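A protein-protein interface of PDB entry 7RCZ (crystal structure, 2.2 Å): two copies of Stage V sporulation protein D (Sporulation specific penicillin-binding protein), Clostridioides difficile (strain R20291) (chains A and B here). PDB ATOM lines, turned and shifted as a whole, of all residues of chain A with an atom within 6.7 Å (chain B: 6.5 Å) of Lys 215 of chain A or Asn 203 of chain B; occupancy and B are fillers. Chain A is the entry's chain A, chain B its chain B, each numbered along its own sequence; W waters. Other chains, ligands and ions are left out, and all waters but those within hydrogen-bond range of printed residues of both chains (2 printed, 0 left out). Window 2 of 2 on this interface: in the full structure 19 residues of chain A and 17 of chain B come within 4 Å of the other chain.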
ATOM      1  N   MET A 212      11.575  26.524 -18.073  1.00  0.00           N
ATOM      2  CA  MET A 212      10.625  25.395 -17.943  1.00  0.00           C
ATOM      3  C   MET A 212      10.367  24.786 -19.323  1.00  0.00           C
ATOM      4  O   MET A 212      10.280  25.538 -20.340  1.00  0.00           O
ATOM      5  CB  MET A 212       9.327  25.879 -17.272  1.00  0.00           C
ATOM      6  CG  MET A 212       8.285  24.821 -17.110  1.00  0.00           C
ATOM      7  SD  MET A 212       6.863  25.389 -16.128  1.00  0.00           S
ATOM      8  CE  MET A 212       7.569  25.403 -14.496  1.00  0.00           C
ATOM      9  N   ASN A 213      10.285  23.454 -19.355  1.00  0.00           N
ATOM     10  CA  ASN A 213       9.675  22.705 -20.470  1.00  0.00           C
ATOM     11  C   ASN A 213       8.161  22.757 -20.308  1.00  0.00           C
ATOM     12  O   ASN A 213       7.630  22.047 -19.454  1.00  0.00           O
ATOM     13  CB  ASN A 213      10.210  21.284 -20.532  1.00  0.00           C
ATOM     14  CG  ASN A 213       9.743  20.567 -21.773  1.00  0.00           C
ATOM     15  OD1 ASN A 213       8.760  20.958 -22.372  1.00  0.00           O
ATOM     16  ND2 ASN A 213      10.413  19.497 -22.144  1.00  0.00           N
ATOM     17  N   PRO A 214       7.431  23.546 -21.138  1.00  0.00           N
ATOM     18  CA  PRO A 214       5.983  23.706 -20.974  1.00  0.00           C
ATOM     19  C   PRO A 214       5.222  22.396 -21.279  1.00  0.00           C
ATOM     20  O   PRO A 214       4.171  22.178 -20.737  1.00  0.00           O
ATOM     21  CB  PRO A 214       5.624  24.851 -21.945  1.00  0.00           C
ATOM     22  CG  PRO A 214       6.704  24.750 -23.043  1.00  0.00           C
ATOM     23  CD  PRO A 214       7.945  24.285 -22.312  1.00  0.00           C
ATOM     24  N   LYS A 215       5.795  21.498 -22.078  1.00  0.00           N
ATOM     25  CA  LYS A 215       5.124  20.219 -22.439  1.00  0.00           C
ATOM     26  C   LYS A 215       5.093  19.246 -21.257  1.00  0.00           C
ATOM     27  O   LYS A 215       4.188  18.404 -21.245  1.00  0.00           O
ATOM     28  CB  LYS A 215       5.791  19.549 -23.643  1.00  0.00           C
ATOM     29  CG  LYS A 215       5.760  20.423 -24.881  1.00  0.00           C
ATOM     30  CD  LYS A 215       5.985  19.690 -26.174  1.00  0.00           C
ATOM     31  CE  LYS A 215       6.645  20.581 -27.201  1.00  0.00           C
ATOM     32  NZ  LYS A 215       6.212  20.235 -28.569  1.00  0.00           N
ATOM     33  N   THR A 216       6.052  19.329 -20.329  1.00  0.00           N
ATOM     34  CA  THR A 216       6.205  18.326 -19.237  1.00  0.00           C
ATOM     35  C   THR A 216       6.078  18.985 -17.860  1.00  0.00           C
ATOM     36  O   THR A 216       5.883  18.239 -16.926  1.00  0.00           O
ATOM     37  CB  THR A 216       7.545  17.596 -19.371  1.00  0.00           C
ATOM     38  OG1 THR A 216       8.581  18.567 -19.210  1.00  0.00           O
ATOM     39  CG2 THR A 216       7.734  16.916 -20.712  1.00  0.00           C
ATOM     40  N   GLY A 217       6.256  20.314 -17.742  1.00  0.00           N
ATOM     41  CA  GLY A 217       6.422  20.995 -16.447  1.00  0.00           C
ATOM     42  C   GLY A 217       7.806  20.818 -15.827  1.00  0.00           C
ATOM     43  O   GLY A 217       8.031  21.347 -14.700  1.00  0.00           O
ATOM     44  N   ASP A 218       8.725  20.142 -16.518  1.00  0.00           N
ATOM     45  CA  ASP A 218      10.135  19.990 -16.082  1.00  0.00           C
ATOM     46  C   ASP A 218      10.785  21.375 -15.924  1.00  0.00           C
ATOM     47  O   ASP A 218      10.695  22.190 -16.859  1.00  0.00           O
ATOM     48  CB  ASP A 218      10.929  19.148 -17.071  1.00  0.00           C
ATOM     49  CG  ASP A 218      10.476  17.693 -17.126  1.00  0.00           C
ATOM     50  OD1 ASP A 218       9.890  17.199 -16.125  1.00  0.00           O
ATOM     51  OD2 ASP A 218      10.732  17.057 -18.164  1.00  0.00           O
ATOM     52  N   SER A 404       3.173  28.651 -18.928  1.00  0.00           N
ATOM     53  CA  SER A 404       3.530  27.397 -19.642  1.00  0.00           C
ATOM     54  C   SER A 404       2.272  26.673 -20.136  1.00  0.00           C
ATOM     55  O   SER A 404       2.373  26.034 -21.206  1.00  0.00           O
ATOM     56  CB  SER A 404       4.393  26.480 -18.818  1.00  0.00           C
ATOM     57  OG  SER A 404       5.663  27.058 -18.580  1.00  0.00           O
ATOM     58  N   ALA A 407       1.364  27.978 -23.426  1.00  0.00           N
ATOM     59  CA  ALA A 407       2.342  27.482 -24.422  1.00  0.00           C
ATOM     60  C   ALA A 407       2.236  25.957 -24.606  1.00  0.00           C
ATOM     61  O   ALA A 407       3.055  25.389 -25.337  1.00  0.00           O
ATOM     62  CB  ALA A 407       3.719  27.823 -23.952  1.00  0.00           C
ATOM     63  N   ASN A 408       1.281  25.296 -23.971  1.00  0.00           N
ATOM     64  CA  ASN A 408       1.133  23.817 -24.020  1.00  0.00           C
ATOM     65  C   ASN A 408      -0.310  23.439 -24.367  1.00  0.00           C
ATOM     66  O   ASN A 408      -0.851  22.510 -23.711  1.00  0.00           O
ATOM     67  CB  ASN A 408       1.533  23.242 -22.662  1.00  0.00           C
ATOM     68  CG  ASN A 408       1.589  21.735 -22.645  1.00  0.00           C
ATOM     69  OD1 ASN A 408       2.051  21.124 -23.613  1.00  0.00           O
ATOM     70  ND2 ASN A 408       1.125  21.154 -21.542  1.00  0.00           N
ATOM     71  N   MET A 413       0.417  21.892 -16.166  1.00  0.00           N
ATOM     72  CA  MET A 413       1.248  20.739 -15.759  1.00  0.00           C
ATOM     73  C   MET A 413       1.792  20.996 -14.359  1.00  0.00           C
ATOM     74  O   MET A 413       2.020  22.157 -14.001  1.00  0.00           O
ATOM     75  CB  MET A 413       2.421  20.545 -16.725  1.00  0.00           C
ATOM     76  CG  MET A 413       2.008  20.434 -18.168  1.00  0.00           C
ATOM     77  SD  MET A 413       0.872  19.054 -18.520  1.00  0.00           S
ATOM     78  CE  MET A 413       1.981  17.640 -18.504  1.00  0.00           C
ATOM     79  N   PRO A 434       5.066  13.060 -16.700  1.00  0.00           N
ATOM     80  CA  PRO A 434       4.456  14.377 -16.577  1.00  0.00           C
ATOM     81  C   PRO A 434       3.023  14.244 -16.055  1.00  0.00           C
ATOM     82  O   PRO A 434       2.343  13.340 -16.472  1.00  0.00           O
ATOM     83  CB  PRO A 434       4.426  14.900 -18.023  1.00  0.00           C
ATOM     84  CG  PRO A 434       5.556  14.162 -18.719  1.00  0.00           C
ATOM     85  CD  PRO A 434       5.584  12.801 -18.051  1.00  0.00           C
ATOM     86  N   ASP A 504       5.773  26.052 -31.744  1.00  0.00           N
ATOM     87  CA  ASP A 504       5.864  24.744 -31.053  1.00  0.00           C
ATOM     88  C   ASP A 504       6.710  24.898 -29.797  1.00  0.00           C
ATOM     89  O   ASP A 504       7.879  24.556 -29.779  1.00  0.00           O
ATOM     90  CB  ASP A 504       6.401  23.688 -32.024  1.00  0.00           C
ATOM     91  CG  ASP A 504       6.557  22.338 -31.361  1.00  0.00           C
ATOM     92  OD1 ASP A 504       5.791  22.070 -30.400  1.00  0.00           O
ATOM     93  OD2 ASP A 504       7.467  21.605 -31.776  1.00  0.00           O
ATOM     94  N   PRO A 505       6.151  25.461 -28.718  1.00  0.00           N
ATOM     95  CA  PRO A 505       6.974  25.930 -27.601  1.00  0.00           C
ATOM     96  C   PRO A 505       7.719  24.800 -26.890  1.00  0.00           C
ATOM     97  O   PRO A 505       7.162  23.739 -26.681  1.00  0.00           O
ATOM     98  CB  PRO A 505       5.968  26.661 -26.694  1.00  0.00           C
ATOM     99  CG  PRO A 505       4.844  27.047 -27.662  1.00  0.00           C
ATOM    100  CD  PRO A 505       4.746  25.868 -28.597  1.00  0.00           C
ATOM    101  N   GLN A 506       9.013  25.029 -26.650  1.00  0.00           N
ATOM    102  CA  GLN A 506       9.937  24.019 -26.089  1.00  0.00           C
ATOM    103  C   GLN A 506      10.525  24.563 -24.803  1.00  0.00           C
ATOM    104  O   GLN A 506      10.933  23.775 -23.999  1.00  0.00           O
ATOM    105  CB  GLN A 506      10.954  23.629 -27.169  1.00  0.00           C
ATOM    106  CG  GLN A 506      10.302  22.785 -28.252  1.00  0.00           C
ATOM    107  CD  GLN A 506      11.036  22.735 -29.565  1.00  0.00           C
ATOM    108  OE1 GLN A 506      10.495  23.110 -30.624  1.00  0.00           O
ATOM    109  NE2 GLN A 506      12.261  22.263 -29.485  1.00  0.00           N
ATOM    110  N   ALA B 198       5.217   6.835 -26.309  1.00  0.00           N
ATOM    111  CA  ALA B 198       6.631   7.258 -26.315  1.00  0.00           C
ATOM    112  C   ALA B 198       6.805   8.416 -27.283  1.00  0.00           C
ATOM    113  O   ALA B 198       7.665   9.260 -27.006  1.00  0.00           O
ATOM    114  CB  ALA B 198       7.561   6.135 -26.690  1.00  0.00           C
ATOM    115  N   TYR B 199       6.124   8.370 -28.434  1.00  0.00           N
ATOM    116  CA  TYR B 199       6.222   9.412 -29.485  1.00  0.00           C
ATOM    117  C   TYR B 199       5.828  10.767 -28.876  1.00  0.00           C
ATOM    118  O   TYR B 199       6.546  11.722 -29.109  1.00  0.00           O
ATOM    119  CB  TYR B 199       5.347   9.075 -30.684  1.00  0.00           C
ATOM    120  CG  TYR B 199       5.364  10.115 -31.780  1.00  0.00           C
ATOM    121  CD1 TYR B 199       6.539  10.453 -32.433  1.00  0.00           C
ATOM    122  CD2 TYR B 199       4.192  10.749 -32.173  1.00  0.00           C
ATOM    123  CE1 TYR B 199       6.549  11.381 -33.465  1.00  0.00           C
ATOM    124  CE2 TYR B 199       4.183  11.665 -33.214  1.00  0.00           C
ATOM    125  CZ  TYR B 199       5.368  11.997 -33.848  1.00  0.00           C
ATOM    126  OH  TYR B 199       5.354  12.930 -34.836  1.00  0.00           O
ATOM    127  N   GLU B 200       4.742  10.802 -28.102  1.00  0.00           N
ATOM    128  CA  GLU B 200       4.181  11.990 -27.403  1.00  0.00           C
ATOM    129  C   GLU B 200       5.112  12.408 -26.248  1.00  0.00           C
ATOM    130  O   GLU B 200       5.531  13.579 -26.221  1.00  0.00           O
ATOM    131  CB  GLU B 200       2.783  11.670 -26.850  1.00  0.00           C
ATOM    132  CG  GLU B 200       1.653  11.753 -27.879  1.00  0.00           C
ATOM    133  CD  GLU B 200       0.349  11.092 -27.430  1.00  0.00           C
ATOM    134  OE1 GLU B 200       0.034  11.162 -26.216  1.00  0.00           O
ATOM    135  OE2 GLU B 200      -0.341  10.476 -28.278  1.00  0.00           O
ATOM    136  N   LEU B 201       5.460  11.473 -25.360  1.00  0.00           N
ATOM    137  CA  LEU B 201       6.238  11.736 -24.122  1.00  0.00           C
ATOM    138  C   LEU B 201       7.614  12.321 -24.458  1.00  0.00           C
ATOM    139  O   LEU B 201       8.047  13.194 -23.729  1.00  0.00           O
ATOM    140  CB  LEU B 201       6.366  10.432 -23.334  1.00  0.00           C
ATOM    141  CG  LEU B 201       6.929  10.568 -21.923  1.00  0.00           C
ATOM    142  CD1 LEU B 201       5.996  11.385 -21.067  1.00  0.00           C
ATOM    143  CD2 LEU B 201       7.141   9.207 -21.274  1.00  0.00           C
ATOM    144  N   ASN B 202       8.230  11.899 -25.564  1.00  0.00           N
ATOM    145  CA  ASN B 202       9.639  12.171 -25.916  1.00  0.00           C
ATOM    146  C   ASN B 202       9.731  13.220 -27.015  1.00  0.00           C
ATOM    147  O   ASN B 202      10.886  13.538 -27.415  1.00  0.00           O
ATOM    148  CB  ASN B 202      10.336  10.890 -26.380  1.00  0.00           C
ATOM    149  CG  ASN B 202      10.529   9.920 -25.238  1.00  0.00           C
ATOM    150  OD1 ASN B 202      11.364  10.163 -24.360  1.00  0.00           O
ATOM    151  ND2 ASN B 202       9.702   8.883 -25.197  1.00  0.00           N
ATOM    152  N   ASN B 203       8.582  13.682 -27.529  1.00  0.00           N
ATOM    153  CA  ASN B 203       8.505  14.714 -28.603  1.00  0.00           C
ATOM    154  C   ASN B 203       9.538  14.352 -29.673  1.00  0.00           C
ATOM    155  O   ASN B 203      10.257  15.237 -30.118  1.00  0.00           O
ATOM    156  CB  ASN B 203       8.674  16.129 -28.012  1.00  0.00           C
ATOM    157  CG  ASN B 203       8.316  17.273 -28.950  1.00  0.00           C
ATOM    158  OD1 ASN B 203       7.455  17.132 -29.833  1.00  0.00           O
ATOM    159  ND2 ASN B 203       8.950  18.428 -28.742  1.00  0.00           N
ATOM    160  N   ALA B 204       9.579  13.086 -30.091  1.00  0.00           N
ATOM    161  CA  ALA B 204      10.634  12.498 -30.954  1.00  0.00           C
ATOM    162  C   ALA B 204      10.358  12.788 -32.424  1.00  0.00           C
ATOM    163  O   ALA B 204       9.214  13.124 -32.772  1.00  0.00           O
ATOM    164  CB  ALA B 204      10.718  11.010 -30.728  1.00  0.00           C
ATOM    165  N   LYS B 205      11.380  12.654 -33.264  1.00  0.00           N
ATOM    166  CA  LYS B 205      11.193  12.666 -34.727  1.00  0.00           C
ATOM    167  C   LYS B 205      10.420  11.382 -35.102  1.00  0.00           C
ATOM    168  O   LYS B 205       9.442  11.505 -35.867  1.00  0.00           O
ATOM    169  CB  LYS B 205      12.522  12.776 -35.469  1.00  0.00           C
ATOM    170  CG  LYS B 205      12.373  12.723 -36.983  1.00  0.00           C
ATOM    171  CD  LYS B 205      13.636  13.049 -37.770  1.00  0.00           C
ATOM    172  CE  LYS B 205      13.325  13.801 -39.054  1.00  0.00           C
ATOM    173  NZ  LYS B 205      14.542  14.123 -39.840  1.00  0.00           N
ATOM    174  N   ASP B 514      13.989   7.971 -31.947  1.00  0.00           N
ATOM    175  CA  ASP B 514      14.871   8.745 -32.860  1.00  0.00           C
ATOM    176  C   ASP B 514      14.694  10.248 -32.565  1.00  0.00           C
ATOM    177  O   ASP B 514      13.592  10.766 -32.803  1.00  0.00           O
ATOM    178  CB  ASP B 514      14.558   8.349 -34.301  1.00  0.00           C
ATOM    179  CG  ASP B 514      15.389   9.060 -35.356  1.00  0.00           C
ATOM    180  OD1 ASP B 514      15.918  10.149 -35.044  1.00  0.00           O
ATOM    181  OD2 ASP B 514      15.491   8.519 -36.485  1.00  0.00           O
ATOM    182  N   GLU B 515      15.746  10.916 -32.060  1.00  0.00           N
ATOM    183  CA  GLU B 515      15.756  12.376 -31.716  1.00  0.00           C
ATOM    184  C   GLU B 515      14.722  12.698 -30.650  1.00  0.00           C
ATOM    185  O   GLU B 515      13.798  13.474 -30.878  1.00  0.00           O
ATOM    186  CB  GLU B 515      15.447  13.256 -32.931  1.00  0.00           C
ATOM    187  CG  GLU B 515      16.604  13.279 -33.902  1.00  0.00           C
ATOM    188  CD  GLU B 515      16.416  14.201 -35.089  1.00  0.00           C
ATOM    189  OE1 GLU B 515      15.424  14.985 -35.086  1.00  0.00           O
ATOM    190  OE2 GLU B 515      17.245  14.116 -36.022  1.00  0.00           O
ATOM    191  N   PRO B 516      14.831  12.133 -29.444  1.00  0.00           N
ATOM    192  CA  PRO B 516      13.969  12.576 -28.365  1.00  0.00           C
ATOM    193  C   PRO B 516      14.286  14.067 -28.148  1.00  0.00           C
ATOM    194  O   PRO B 516      15.444  14.454 -28.394  1.00  0.00           O
ATOM    195  CB  PRO B 516      14.348  11.635 -27.212  1.00  0.00           C
ATOM    196  CG  PRO B 516      15.756  11.220 -27.513  1.00  0.00           C
ATOM    197  CD  PRO B 516      15.877  11.212 -29.015  1.00  0.00           C
ATOM    198  N   THR B 517      13.282  14.873 -27.776  1.00  0.00           N
ATOM    199  CA  THR B 517      13.379  16.361 -27.666  1.00  0.00           C
ATOM    200  C   THR B 517      12.832  16.810 -26.307  1.00  0.00           C
ATOM    201  O   THR B 517      11.698  16.420 -25.963  1.00  0.00           O
ATOM    202  CB  THR B 517      12.656  17.037 -28.840  1.00  0.00           C
ATOM    203  OG1 THR B 517      13.287  16.585 -30.040  1.00  0.00           O
ATOM    204  CG2 THR B 517      12.704  18.550 -28.806  1.00  0.00           C
ATOM    205  N   GLY B 518      13.623  17.574 -25.555  1.00  0.00           N
ATOM    206  CA  GLY B 518      13.225  18.188 -24.279  1.00  0.00           C
ATOM    207  C   GLY B 518      13.357  17.237 -23.106  1.00  0.00           C
ATOM    208  O   GLY B 518      12.909  17.572 -21.999  1.00  0.00           O
ATOM    209  N   VAL B 519      13.935  16.078 -23.355  1.00  0.00           N
ATOM    210  CA  VAL B 519      14.045  15.066 -22.283  1.00  0.00           C
ATOM    211  C   VAL B 519      15.440  14.462 -22.320  1.00  0.00           C
ATOM    212  O   VAL B 519      16.128  14.612 -23.316  1.00  0.00           O
ATOM    213  CB  VAL B 519      12.978  13.974 -22.465  1.00  0.00           C
ATOM    214  CG1 VAL B 519      11.583  14.448 -22.111  1.00  0.00           C
ATOM    215  CG2 VAL B 519      13.009  13.388 -23.854  1.00  0.00           C
HETATM  216  O   HOH W   1       6.337  18.894 -31.390  1.00  0.00           O
HETATM  217  O   HOH W   2       9.492  17.704 -24.398  1.00  0.00           O
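CD1 of Leu 201 of chain B touches CD of Pro 434 of chain A (3.4 Å). CG2 of Thr 517 of chain B touches NE2 of Gln 506 of chain A, at 3.8 Å.
Lys 215 of chain A touches just one residue of chain B: Asn 203 (3.3 Å). Of the printed residues of chain B, Asn 213 of chain A touches Gly 518. Printed residues of chain A within 4 Å of Leu 201 of chain B: Pro 434 (3.4 Å). Of the printed residues of chain A, Gly 518 of chain B touches Asn 213. Of the printed residues of chain B, Gln 506 of chain A touches Thr 517. Ser 404 of chain A touches none of the printed residues of chain B. Pro 516 of chain B touches none of the printed residues of chain A. The nearest residue of chain B that does not touch Lys 215 of chain A is Glu 200 of chain B (6.1 Å). The nearest residue of chain A that does not touch Asn 203 of chain B is Gln 506 of chain A (4.6 Å). The nearest printed residue of chain B that does not touch Pro 434 of chain A is Val 519 of chain B (6.9 Å).
Of the 14 printed residues of chain B, 4 touch a printed residue of chain A. Of the 15 printed residues of chain A, 4 touch a printed residue of chain B. Hydrophobic or aromatic side chains of chain A that line the printed part of chain B: Pro 434. Among the printed residues, no Asp or Glu carboxylate lies within 4 Å of a Lys or Arg side-chain nitrogen of the other chain.
The side-chain amide nitrogen (ND2) of Asn 213 of chain A lies within hydrogen-bond range of the backbone carbonyl oxygen (O) of Gly 518 of chain B. The side-chain amino group (NZ) of Lys 215 of chain A lies close to the side-chain amide nitrogen (ND2) of Asn 203 of chain B (3.3 Å).
No position is printed for both chains.
N of Asn 213 of chain A sits at hydrogen-bond distance from O of Asp 218 of chain A, 2.8 Å away. OD1 of Asp 504 of chain A is in salt-bridge range of NZ of Lys 215 of chain A. The backbone carbonyl oxygen (O) of Asn 203 of chain B sits close to the side-chain hydroxyl (OG1) of Thr 517 of chain B (3.3 Å). The backbone carbonyl oxygen (O) of Asn 202 of chain B is in hydrogen-bond range of the backbone NH (N) of Thr 517 of chain B (2.8 Å). OD1 of Asn 213 of chain A is in hydrogen-bond range of N of Lys 215 of chain A (3.0 Å). OE1 of Gln 506 of chain A sits close to O of Asp 504 of chain A (3.1 Å).
Water W1 lies within hydrogen-bond range of OD1 of Asn 203 of chain B (2.6 Å), OD2 of Asp 504 of chain A (3.0 Å) and NZ of Lys 215 of chain A (3.1 Å). Water W2 lies within hydrogen-bond range of the backbone carbonyl oxygen (O) of Thr 517 of chain B (3.0 Å) and the side-chain amide nitrogen (ND2) of Asn 213 of chain A (3.0 Å).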
